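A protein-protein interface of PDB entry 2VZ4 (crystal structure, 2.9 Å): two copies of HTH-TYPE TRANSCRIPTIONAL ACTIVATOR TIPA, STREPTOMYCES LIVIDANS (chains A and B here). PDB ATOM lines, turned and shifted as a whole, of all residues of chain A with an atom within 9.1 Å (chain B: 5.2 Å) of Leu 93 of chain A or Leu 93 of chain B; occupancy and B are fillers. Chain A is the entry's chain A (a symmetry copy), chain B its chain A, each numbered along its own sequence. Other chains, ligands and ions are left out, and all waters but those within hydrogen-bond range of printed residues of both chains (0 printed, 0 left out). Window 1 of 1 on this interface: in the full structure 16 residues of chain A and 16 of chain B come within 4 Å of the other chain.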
ATOM      1  N   PHE A  53     -36.731 -17.015  -3.901  1.00  0.00           N
ATOM      2  CA  PHE A  53     -35.333 -17.350  -4.179  1.00  0.00           C
ATOM      3  C   PHE A  53     -34.428 -16.139  -4.007  1.00  0.00           C
ATOM      4  O   PHE A  53     -33.432 -16.168  -3.268  1.00  0.00           O
ATOM      5  CB  PHE A  53     -35.164 -17.877  -5.599  1.00  0.00           C
ATOM      6  CG  PHE A  53     -33.765 -18.297  -5.907  1.00  0.00           C
ATOM      7  CD1 PHE A  53     -33.338 -19.592  -5.628  1.00  0.00           C
ATOM      8  CD2 PHE A  53     -32.856 -17.390  -6.452  1.00  0.00           C
ATOM      9  CE1 PHE A  53     -32.031 -19.986  -5.902  1.00  0.00           C
ATOM     10  CE2 PHE A  53     -31.542 -17.767  -6.727  1.00  0.00           C
ATOM     11  CZ  PHE A  53     -31.126 -19.069  -6.454  1.00  0.00           C
ATOM     12  N   GLU A  56     -34.204 -14.731  -0.500  1.00  0.00           N
ATOM     13  CA  GLU A  56     -33.234 -15.459   0.343  1.00  0.00           C
ATOM     14  C   GLU A  56     -31.776 -15.087   0.096  1.00  0.00           C
ATOM     15  O   GLU A  56     -30.929 -15.225   0.988  1.00  0.00           O
ATOM     16  CB  GLU A  56     -33.371 -16.977   0.197  1.00  0.00           C
ATOM     17  CG  GLU A  56     -34.168 -17.639   1.322  1.00  0.00           C
ATOM     18  CD  GLU A  56     -33.484 -18.892   1.885  1.00  0.00           C
ATOM     19  OE1 GLU A  56     -34.032 -20.010   1.695  1.00  0.00           O
ATOM     20  OE2 GLU A  56     -32.406 -18.748   2.521  1.00  0.00           O
ATOM     21  N   LEU A  57     -31.473 -14.641  -1.118  1.00  0.00           N
ATOM     22  CA  LEU A  57     -30.140 -14.126  -1.417  1.00  0.00           C
ATOM     23  C   LEU A  57     -30.108 -12.597  -1.259  1.00  0.00           C
ATOM     24  O   LEU A  57     -29.276 -11.926  -1.864  1.00  0.00           O
ATOM     25  CB  LEU A  57     -29.695 -14.575  -2.820  1.00  0.00           C
ATOM     26  CG  LEU A  57     -29.608 -16.094  -3.042  1.00  0.00           C
ATOM     27  CD1 LEU A  57     -29.372 -16.405  -4.504  1.00  0.00           C
ATOM     28  CD2 LEU A  57     -28.513 -16.728  -2.185  1.00  0.00           C
ATOM     29  N   GLN A  82     -28.805 -17.590 -11.241  1.00  0.00           N
ATOM     30  CA  GLN A  82     -29.185 -18.208  -9.970  1.00  0.00           C
ATOM     31  C   GLN A  82     -28.112 -19.179  -9.496  1.00  0.00           C
ATOM     32  O   GLN A  82     -27.826 -19.269  -8.297  1.00  0.00           O
ATOM     33  CB  GLN A  82     -30.529 -18.912 -10.106  1.00  0.00           C
ATOM     34  CG  GLN A  82     -31.674 -17.935 -10.320  1.00  0.00           C
ATOM     35  CD  GLN A  82     -32.991 -18.615 -10.602  1.00  0.00           C
ATOM     36  OE1 GLN A  82     -33.061 -19.840 -10.691  1.00  0.00           O
ATOM     37  NE2 GLN A  82     -34.047 -17.821 -10.748  1.00  0.00           N
ATOM     38  N   HIS A  83     -27.504 -19.884 -10.447  1.00  0.00           N
ATOM     39  CA  HIS A  83     -26.380 -20.770 -10.156  1.00  0.00           C
ATOM     40  C   HIS A  83     -25.141 -19.987  -9.696  1.00  0.00           C
ATOM     41  O   HIS A  83     -24.479 -20.363  -8.721  1.00  0.00           O
ATOM     42  CB  HIS A  83     -26.038 -21.614 -11.389  1.00  0.00           C
ATOM     43  CG  HIS A  83     -25.229 -22.832 -11.074  1.00  0.00           C
ATOM     44  ND1 HIS A  83     -23.852 -22.828 -11.066  1.00  0.00           N
ATOM     45  CD2 HIS A  83     -25.607 -24.088 -10.739  1.00  0.00           C
ATOM     46  CE1 HIS A  83     -23.416 -24.034 -10.748  1.00  0.00           C
ATOM     47  NE2 HIS A  83     -24.461 -24.818 -10.544  1.00  0.00           N
ATOM     48  N   LEU A  85     -24.987 -17.037  -8.321  1.00  0.00           N
ATOM     49  CA  LEU A  85     -25.222 -16.408  -7.029  1.00  0.00           C
ATOM     50  C   LEU A  85     -25.005 -17.406  -5.906  1.00  0.00           C
ATOM     51  O   LEU A  85     -24.310 -17.112  -4.923  1.00  0.00           O
ATOM     52  CB  LEU A  85     -26.648 -15.845  -6.956  1.00  0.00           C
ATOM     53  CG  LEU A  85     -26.881 -14.506  -7.665  1.00  0.00           C
ATOM     54  CD1 LEU A  85     -28.378 -14.232  -7.859  1.00  0.00           C
ATOM     55  CD2 LEU A  85     -26.206 -13.364  -6.902  1.00  0.00           C
ATOM     56  N   LEU A  86     -25.605 -18.584  -6.060  1.00  0.00           N
ATOM     57  CA  LEU A  86     -25.438 -19.664  -5.090  1.00  0.00           C
ATOM     58  C   LEU A  86     -23.974 -20.104  -4.972  1.00  0.00           C
ATOM     59  O   LEU A  86     -23.501 -20.433  -3.886  1.00  0.00           O
ATOM     60  CB  LEU A  86     -26.327 -20.861  -5.452  1.00  0.00           C
ATOM     61  CG  LEU A  86     -27.832 -20.677  -5.226  1.00  0.00           C
ATOM     62  CD1 LEU A  86     -28.598 -21.827  -5.851  1.00  0.00           C
ATOM     63  CD2 LEU A  86     -28.170 -20.552  -3.737  1.00  0.00           C
ATOM     64  N   SER A  87     -23.257 -20.094  -6.087  1.00  0.00           N
ATOM     65  CA  SER A  87     -21.862 -20.514  -6.087  1.00  0.00           C
ATOM     66  C   SER A  87     -20.990 -19.486  -5.359  1.00  0.00           C
ATOM     67  O   SER A  87     -20.200 -19.849  -4.492  1.00  0.00           O
ATOM     68  CB  SER A  87     -21.396 -20.764  -7.519  1.00  0.00           C
ATOM     69  OG  SER A  87     -22.313 -21.636  -8.175  1.00  0.00           O
ATOM     70  N   ALA A  88     -21.166 -18.214  -5.701  1.00  0.00           N
ATOM     71  CA  ALA A  88     -20.574 -17.101  -4.961  1.00  0.00           C
ATOM     72  C   ALA A  88     -20.762 -17.275  -3.461  1.00  0.00           C
ATOM     73  O   ALA A  88     -19.809 -17.192  -2.673  1.00  0.00           O
ATOM     74  CB  ALA A  88     -21.232 -15.800  -5.391  1.00  0.00           C
ATOM     75  N   ARG A  89     -22.012 -17.521  -3.086  1.00  0.00           N
ATOM     76  CA  ARG A  89     -22.432 -17.565  -1.691  1.00  0.00           C
ATOM     77  C   ARG A  89     -21.914 -18.818  -0.982  1.00  0.00           C
ATOM     78  O   ARG A  89     -21.508 -18.756   0.177  1.00  0.00           O
ATOM     79  CB  ARG A  89     -23.968 -17.493  -1.629  1.00  0.00           C
ATOM     80  CG  ARG A  89     -24.585 -17.246  -0.249  1.00  0.00           C
ATOM     81  CD  ARG A  89     -24.102 -15.943   0.369  1.00  0.00           C
ATOM     82  NE  ARG A  89     -24.919 -15.492   1.502  1.00  0.00           N
ATOM     83  CZ  ARG A  89     -24.987 -16.082   2.701  1.00  0.00           C
ATOM     84  NH1 ARG A  89     -24.316 -17.196   2.950  1.00  0.00           N
ATOM     85  NH2 ARG A  89     -25.745 -15.566   3.668  1.00  0.00           N
ATOM     86  N   ILE A  90     -21.929 -19.953  -1.676  1.00  0.00           N
ATOM     87  CA  ILE A  90     -21.384 -21.188  -1.116  1.00  0.00           C
ATOM     88  C   ILE A  90     -19.902 -20.983  -0.838  1.00  0.00           C
ATOM     89  O   ILE A  90     -19.417 -21.250   0.261  1.00  0.00           O
ATOM     90  CB  ILE A  90     -21.608 -22.406  -2.047  1.00  0.00           C
ATOM     91  CG1 ILE A  90     -23.077 -22.837  -1.994  1.00  0.00           C
ATOM     92  CG2 ILE A  90     -20.729 -23.569  -1.619  1.00  0.00           C
ATOM     93  CD1 ILE A  90     -23.477 -23.845  -3.034  1.00  0.00           C
ATOM     94  N   GLY A  91     -19.193 -20.468  -1.831  1.00  0.00           N
ATOM     95  CA  GLY A  91     -17.778 -20.181  -1.680  1.00  0.00           C
ATOM     96  C   GLY A  91     -17.484 -19.219  -0.553  1.00  0.00           C
ATOM     97  O   GLY A  91     -16.476 -19.362   0.122  1.00  0.00           O
ATOM     98  N   LYS A  92     -18.357 -18.237  -0.346  1.00  0.00           N
ATOM     99  CA  LYS A  92     -18.161 -17.245   0.722  1.00  0.00           C
ATOM    100  C   LYS A  92     -18.206 -17.894   2.111  1.00  0.00           C
ATOM    101  O   LYS A  92     -17.348 -17.648   2.963  1.00  0.00           O
ATOM    102  CB  LYS A  92     -19.226 -16.141   0.627  1.00  0.00           C
ATOM    103  CG  LYS A  92     -19.230 -15.187   1.811  1.00  0.00           C
ATOM    104  CD  LYS A  92     -19.905 -13.867   1.471  1.00  0.00           C
ATOM    105  CE  LYS A  92     -19.632 -12.819   2.555  1.00  0.00           C
ATOM    106  NZ  LYS A  92     -19.791 -11.413   2.067  1.00  0.00           N
ATOM    107  N   LEU A  93     -19.229 -18.717   2.316  1.00  0.00           N
ATOM    108  CA  LEU A  93     -19.427 -19.411   3.572  1.00  0.00           C
ATOM    109  C   LEU A  93     -18.318 -20.412   3.785  1.00  0.00           C
ATOM    110  O   LEU A  93     -17.792 -20.540   4.878  1.00  0.00           O
ATOM    111  CB  LEU A  93     -20.765 -20.142   3.568  1.00  0.00           C
ATOM    112  CG  LEU A  93     -22.013 -19.270   3.467  1.00  0.00           C
ATOM    113  CD1 LEU A  93     -23.233 -20.163   3.324  1.00  0.00           C
ATOM    114  CD2 LEU A  93     -22.136 -18.367   4.682  1.00  0.00           C
ATOM    115  N   GLN A  94     -17.972 -21.132   2.729  1.00  0.00           N
ATOM    116  CA  GLN A  94     -16.849 -22.052   2.783  1.00  0.00           C
ATOM    117  C   GLN A  94     -15.581 -21.356   3.288  1.00  0.00           C
ATOM    118  O   GLN A  94     -14.821 -21.923   4.075  1.00  0.00           O
ATOM    119  CB  GLN A  94     -16.614 -22.674   1.409  1.00  0.00           C
ATOM    120  CG  GLN A  94     -17.674 -23.700   1.024  1.00  0.00           C
ATOM    121  CD  GLN A  94     -17.427 -24.314  -0.341  1.00  0.00           C
ATOM    122  OE1 GLN A  94     -16.894 -23.660  -1.240  1.00  0.00           O
ATOM    123  NE2 GLN A  94     -17.809 -25.576  -0.505  1.00  0.00           N
ATOM    124  N   LYS A  95     -15.362 -20.125   2.847  1.00  0.00           N
ATOM    125  CA  LYS A  95     -14.222 -19.350   3.321  1.00  0.00           C
ATOM    126  C   LYS A  95     -14.424 -18.989   4.784  1.00  0.00           C
ATOM    127  O   LYS A  95     -13.490 -19.060   5.569  1.00  0.00           O
ATOM    128  CB  LYS A  95     -14.020 -18.084   2.485  1.00  0.00           C
ATOM    129  CG  LYS A  95     -12.658 -17.431   2.677  1.00  0.00           C
ATOM    130  CD  LYS A  95     -12.452 -16.260   1.716  1.00  0.00           C
ATOM    131  CE  LYS A  95     -11.621 -16.630   0.502  1.00  0.00           C
ATOM    132  NZ  LYS A  95     -10.156 -16.473   0.775  1.00  0.00           N
ATOM    133  N   MET A  96     -15.643 -18.612   5.156  1.00  0.00           N
ATOM    134  CA  MET A  96     -15.925 -18.299   6.554  1.00  0.00           C
ATOM    135  C   MET A  96     -15.629 -19.530   7.395  1.00  0.00           C
ATOM    136  O   MET A  96     -14.865 -19.454   8.357  1.00  0.00           O
ATOM    137  CB  MET A  96     -17.380 -17.858   6.760  1.00  0.00           C
ATOM    138  CG  MET A  96     -17.778 -16.594   6.006  1.00  0.00           C
ATOM    139  SD  MET A  96     -19.332 -15.898   6.591  1.00  0.00           S
ATOM    140  CE  MET A  96     -18.812 -15.070   8.111  1.00  0.00           C
ATOM    141  N   ALA A  97     -16.232 -20.658   6.996  1.00  0.00           N
ATOM    142  CA  ALA A  97     -16.092 -21.967   7.667  1.00  0.00           C
ATOM    143  C   ALA A  97     -14.640 -22.420   7.700  1.00  0.00           C
ATOM    144  O   ALA A  97     -14.192 -23.040   8.667  1.00  0.00           O
ATOM    145  CB  ALA A  97     -16.945 -23.017   6.969  1.00  0.00           C
ATOM    146  N   ALA A  98     -13.908 -22.110   6.635  1.00  0.00           N
ATOM    147  CA  ALA A  98     -12.466 -22.321   6.607  1.00  0.00           C
ATOM    148  C   ALA A  98     -11.779 -21.540   7.738  1.00  0.00           C
ATOM    149  O   ALA A  98     -10.933 -22.082   8.443  1.00  0.00           O
ATOM    150  CB  ALA A  98     -11.910 -21.911   5.253  1.00  0.00           C
ATOM    151  N   ALA A  99     -12.160 -20.274   7.909  1.00  0.00           N
ATOM    152  CA  ALA A  99     -11.646 -19.432   9.000  1.00  0.00           C
ATOM    153  C   ALA A  99     -11.973 -20.020  10.366  1.00  0.00           C
ATOM    154  O   ALA A  99     -11.186 -19.883  11.297  1.00  0.00           O
ATOM    155  CB  ALA A  99     -12.211 -18.023   8.908  1.00  0.00           C
ATOM    156  N   VAL A 100     -13.137 -20.654  10.490  1.00  0.00           N
ATOM    157  CA  VAL A 100     -13.515 -21.305  11.740  1.00  0.00           C
ATOM    158  C   VAL A 100     -12.559 -22.461  12.052  1.00  0.00           C
ATOM    159  O   VAL A 100     -12.089 -22.582  13.182  1.00  0.00           O
ATOM    160  CB  VAL A 100     -14.973 -21.819  11.699  1.00  0.00           C
ATOM    161  CG1 VAL A 100     -15.314 -22.587  12.963  1.00  0.00           C
ATOM    162  CG2 VAL A 100     -15.939 -20.659  11.506  1.00  0.00           C
ATOM    163  N   GLU A 101     -12.258 -23.287  11.049  1.00  0.00           N
ATOM    164  CA  GLU A 101     -11.410 -24.464  11.245  1.00  0.00           C
ATOM    165  C   GLU A 101      -9.998 -24.088  11.722  1.00  0.00           C
ATOM    166  O   GLU A 101      -9.412 -24.788  12.555  1.00  0.00           O
ATOM    167  CB  GLU A 101     -11.378 -25.340   9.975  1.00  0.00           C
ATOM    168  CG  GLU A 101     -12.688 -26.136   9.735  1.00  0.00           C
ATOM    169  CD  GLU A 101     -12.786 -26.830   8.355  1.00  0.00           C
ATOM    170  OE1 GLU A 101     -11.746 -27.260   7.797  1.00  0.00           O
ATOM    171  OE2 GLU A 101     -13.926 -26.963   7.841  1.00  0.00           O
ATOM    172  N   LEU B  57     -25.728 -14.582   9.464  1.00  0.00           N
ATOM    173  CA  LEU B  57     -26.540 -15.795   9.484  1.00  0.00           C
ATOM    174  C   LEU B  57     -27.935 -15.497  10.057  1.00  0.00           C
ATOM    175  O   LEU B  57     -28.600 -16.391  10.572  1.00  0.00           O
ATOM    176  CB  LEU B  57     -25.818 -16.909  10.263  1.00  0.00           C
ATOM    177  CG  LEU B  57     -24.450 -17.338   9.706  1.00  0.00           C
ATOM    178  CD1 LEU B  57     -23.754 -18.275  10.669  1.00  0.00           C
ATOM    179  CD2 LEU B  57     -24.580 -17.996   8.334  1.00  0.00           C
ATOM    180  N   LEU B  86     -22.641 -22.634   9.613  1.00  0.00           N
ATOM    181  CA  LEU B  86     -22.096 -22.506   8.262  1.00  0.00           C
ATOM    182  C   LEU B  86     -22.269 -23.796   7.453  1.00  0.00           C
ATOM    183  O   LEU B  86     -22.525 -23.756   6.251  1.00  0.00           O
ATOM    184  CB  LEU B  86     -20.618 -22.098   8.308  1.00  0.00           C
ATOM    185  CG  LEU B  86     -20.329 -20.654   8.733  1.00  0.00           C
ATOM    186  CD1 LEU B  86     -18.842 -20.468   8.973  1.00  0.00           C
ATOM    187  CD2 LEU B  86     -20.836 -19.647   7.698  1.00  0.00           C
ATOM    188  N   ARG B  89     -25.858 -24.199   6.438  1.00  0.00           N
ATOM    189  CA  ARG B  89     -26.157 -23.192   5.428  1.00  0.00           C
ATOM    190  C   ARG B  89     -25.496 -23.519   4.088  1.00  0.00           C
ATOM    191  O   ARG B  89     -26.096 -23.321   3.032  1.00  0.00           O
ATOM    192  CB  ARG B  89     -25.703 -21.815   5.944  1.00  0.00           C
ATOM    193  CG  ARG B  89     -26.181 -20.596   5.150  1.00  0.00           C
ATOM    194  CD  ARG B  89     -27.698 -20.513   5.086  1.00  0.00           C
ATOM    195  NE  ARG B  89     -28.197 -19.201   4.658  1.00  0.00           N
ATOM    196  CZ  ARG B  89     -28.077 -18.681   3.431  1.00  0.00           C
ATOM    197  NH1 ARG B  89     -27.431 -19.332   2.477  1.00  0.00           N
ATOM    198  NH2 ARG B  89     -28.597 -17.487   3.148  1.00  0.00           N
ATOM    199  N   ILE B  90     -24.263 -24.015   4.130  1.00  0.00           N
ATOM    200  CA  ILE B  90     -23.575 -24.432   2.910  1.00  0.00           C
ATOM    201  C   ILE B  90     -24.369 -25.558   2.263  1.00  0.00           C
ATOM    202  O   ILE B  90     -24.689 -25.512   1.077  1.00  0.00           O
ATOM    203  CB  ILE B  90     -22.113 -24.871   3.178  1.00  0.00           C
ATOM    204  CG1 ILE B  90     -21.242 -23.641   3.445  1.00  0.00           C
ATOM    205  CG2 ILE B  90     -21.559 -25.628   1.983  1.00  0.00           C
ATOM    206  CD1 ILE B  90     -19.863 -23.943   3.961  1.00  0.00           C
ATOM    207  N   GLY B  91     -24.721 -26.551   3.065  1.00  0.00           N
ATOM    208  CA  GLY B  91     -25.520 -27.664   2.584  1.00  0.00           C
ATOM    209  C   GLY B  91     -26.851 -27.237   2.012  1.00  0.00           C
ATOM    210  O   GLY B  91     -27.315 -27.822   1.046  1.00  0.00           O
ATOM    211  N   LYS B  92     -27.471 -26.220   2.605  1.00  0.00           N
ATOM    212  CA  LYS B  92     -28.773 -25.730   2.129  1.00  0.00           C
ATOM    213  C   LYS B  92     -28.675 -25.151   0.712  1.00  0.00           C
ATOM    214  O   LYS B  92     -29.487 -25.460  -0.166  1.00  0.00           O
ATOM    215  CB  LYS B  92     -29.326 -24.666   3.090  1.00  0.00           C
ATOM    216  CG  LYS B  92     -30.566 -23.954   2.572  1.00  0.00           C
ATOM    217  CD  LYS B  92     -31.359 -23.308   3.698  1.00  0.00           C
ATOM    218  CE  LYS B  92     -32.742 -22.868   3.208  1.00  0.00           C
ATOM    219  NZ  LYS B  92     -33.740 -22.725   4.315  1.00  0.00           N
ATOM    220  N   LEU B  93     -27.672 -24.302   0.517  1.00  0.00           N
ATOM    221  CA  LEU B  93     -27.436 -23.658  -0.760  1.00  0.00           C
ATOM    222  C   LEU B  93     -27.028 -24.689  -1.784  1.00  0.00           C
ATOM    223  O   LEU B  93     -27.482 -24.659  -2.917  1.00  0.00           O
ATOM    224  CB  LEU B  93     -26.329 -22.618  -0.631  1.00  0.00           C
ATOM    225  CG  LEU B  93     -26.614 -21.436   0.290  1.00  0.00           C
ATOM    226  CD1 LEU B  93     -25.360 -20.589   0.415  1.00  0.00           C
ATOM    227  CD2 LEU B  93     -27.779 -20.614  -0.236  1.00  0.00           C
ATOM    228  N   GLN B  94     -26.156 -25.600  -1.380  1.00  0.00           N
ATOM    229  CA  GLN B  94     -25.769 -26.703  -2.242  1.00  0.00           C
ATOM    230  C   GLN B  94     -26.995 -27.456  -2.771  1.00  0.00           C
ATOM    231  O   GLN B  94     -27.042 -27.844  -3.939  1.00  0.00           O
ATOM    232  CB  GLN B  94     -24.833 -27.650  -1.496  1.00  0.00           C
ATOM    233  CG  GLN B  94     -23.436 -27.076  -1.291  1.00  0.00           C
ATOM    234  CD  GLN B  94     -22.514 -28.028  -0.552  1.00  0.00           C
ATOM    235  OE1 GLN B  94     -22.957 -28.802   0.299  1.00  0.00           O
ATOM    236  NE2 GLN B  94     -21.225 -27.980  -0.873  1.00  0.00           N
ATOM    237  N   LYS B  95     -27.989 -27.649  -1.915  1.00  0.00           N
ATOM    238  CA  LYS B  95     -29.227 -28.292  -2.336  1.00  0.00           C
ATOM    239  C   LYS B  95     -29.979 -27.375  -3.289  1.00  0.00           C
ATOM    240  O   LYS B  95     -30.517 -27.834  -4.285  1.00  0.00           O
ATOM    241  CB  LYS B  95     -30.109 -28.648  -1.136  1.00  0.00           C
ATOM    242  CG  LYS B  95     -31.221 -29.636  -1.462  1.00  0.00           C
ATOM    243  CD  LYS B  95     -31.978 -30.068  -0.206  1.00  0.00           C
ATOM    244  CE  LYS B  95     -31.525 -31.418   0.321  1.00  0.00           C
ATOM    245  NZ  LYS B  95     -32.271 -32.538  -0.337  1.00  0.00           N
ATOM    246  N   MET B  96     -30.009 -26.080  -2.992  1.00  0.00           N
ATOM    247  CA  MET B  96     -30.668 -25.132  -3.886  1.00  0.00           C
ATOM    248  C   MET B  96     -29.993 -25.201  -5.247  1.00  0.00           C
ATOM    249  O   MET B  96     -30.662 -25.405  -6.260  1.00  0.00           O
ATOM    250  CB  MET B  96     -30.612 -23.699  -3.343  1.00  0.00           C
ATOM    251  CG  MET B  96     -31.310 -23.496  -2.002  1.00  0.00           C
ATOM    252  SD  MET B  96     -31.573 -21.758  -1.615  1.00  0.00           S
ATOM    253  CE  MET B  96     -33.004 -21.365  -2.647  1.00  0.00           C
ATOM    254  N   ALA B  97     -28.662 -25.049  -5.237  1.00  0.00           N
ATOM    255  CA  ALA B  97     -27.806 -25.074  -6.442  1.00  0.00           C
ATOM    256  C   ALA B  97     -27.933 -26.396  -7.184  1.00  0.00           C
ATOM    257  O   ALA B  97     -27.887 -26.438  -8.415  1.00  0.00           O
ATOM    258  CB  ALA B  97     -26.351 -24.830  -6.066  1.00  0.00           C
ATOM    259  N   ALA B  98     -28.090 -27.477  -6.427  1.00  0.00           N
ATOM    260  CA  ALA B  98     -28.402 -28.778  -7.004  1.00  0.00           C
ATOM    261  C   ALA B  98     -29.715 -28.721  -7.799  1.00  0.00           C
ATOM    262  O   ALA B  98     -29.786 -29.217  -8.920  1.00  0.00           O
ATOM    263  CB  ALA B  98     -28.483 -29.825  -5.904  1.00  0.00           C
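Printed residues of chain B within 4 Å of Phe 53 of chain A: Met 96. Gln 82 of chain A touches none of the printed residues of chain B. Ala 88 of chain A touches none of the printed residues of chain B. Leu 93 of chain A touches just these residues of chain B: Leu 86, Arg 89, Ile 90 and Leu 93. Printed residues of chain B within 4 Å of Met 96 of chain A: Leu 86 (3.7 Å). No residue of chain A comes within 4 Å of Gly 91 of chain B. The nearest residue of chain A that does not touch Leu 93 of chain B is Leu 57 of chain A (4.4 Å). The nearest printed residue of chain A that does not touch Leu 86 of chain B is Ala 98 of chain A (5.7 Å).
The guanidinium group of Arg 89 of chain B lies close to the guanidinium group of Arg 89 of chain A, 3.5 Å away. The side-chain carboxylate (OE1) of Glu 56 of chain A is in salt-bridge range of the side-chain amino group (NZ) of Lys 92 of chain B (3.8 Å).
Leu 86 of chain A touches Leu 93 of chain B, and with the chains exchanged Leu 93 of chain A touches Leu 86 of chain B. Arg 89 of chain A touches its own counterpart, Arg 89 of chain B. Arg 89 of chain A touches Leu 93 of chain B, and with the chains exchanged Leu 93 of chain A touches Arg 89 of chain B. Leu 93 of chain A touches its own counterpart, Leu 93 of chain B. Of the 18 pairs that touch across the chains among the printed residues, 14 have their exchanged pair printed and touching as well.
Hydrophobic or aromatic side chains of chain B that line the printed part of chain A: Leu 86, Ile 90, Leu 93, Met 96 and Ala 97. Among the printed residues, Asp or Glu carboxylates within 4 Å of a Lys or Arg side-chain nitrogen of the other chain: Glu 56 of chain A with Lys 92 of chain B (3.8 Å).
CE of Met 96 of chain B touches CD1 of Phe 53 of chain A, 3.5 Å away. Glu 56 of chain A touches Arg 89 of chain B (O to NH2, 3.9 Å). Ala 97 of chain B touches Leu 86 of chain A (N to CD1, 3.3 Å). CD1 of Leu 93 of chain B touches CG of Arg 89 of chain A (3.5 Å). Leu 93 of chain B touches Ile 90 of chain A. Leu 93 of chain A touches Leu 86 of chain B. CG1 of Ile 90 of chain B touches CB of Leu 93 of chain A, at 3.5 Å. CD1 of Ile 90 of chain B touches N of Gln 94 of chain A, 3.6 Å away. C of Met 96 of chain A touches CD1 of Leu 86 of chain B (3.7 Å). CD1 of Leu 86 of chain B touches N of Ala 97 of chain A, at 3.3 Å.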
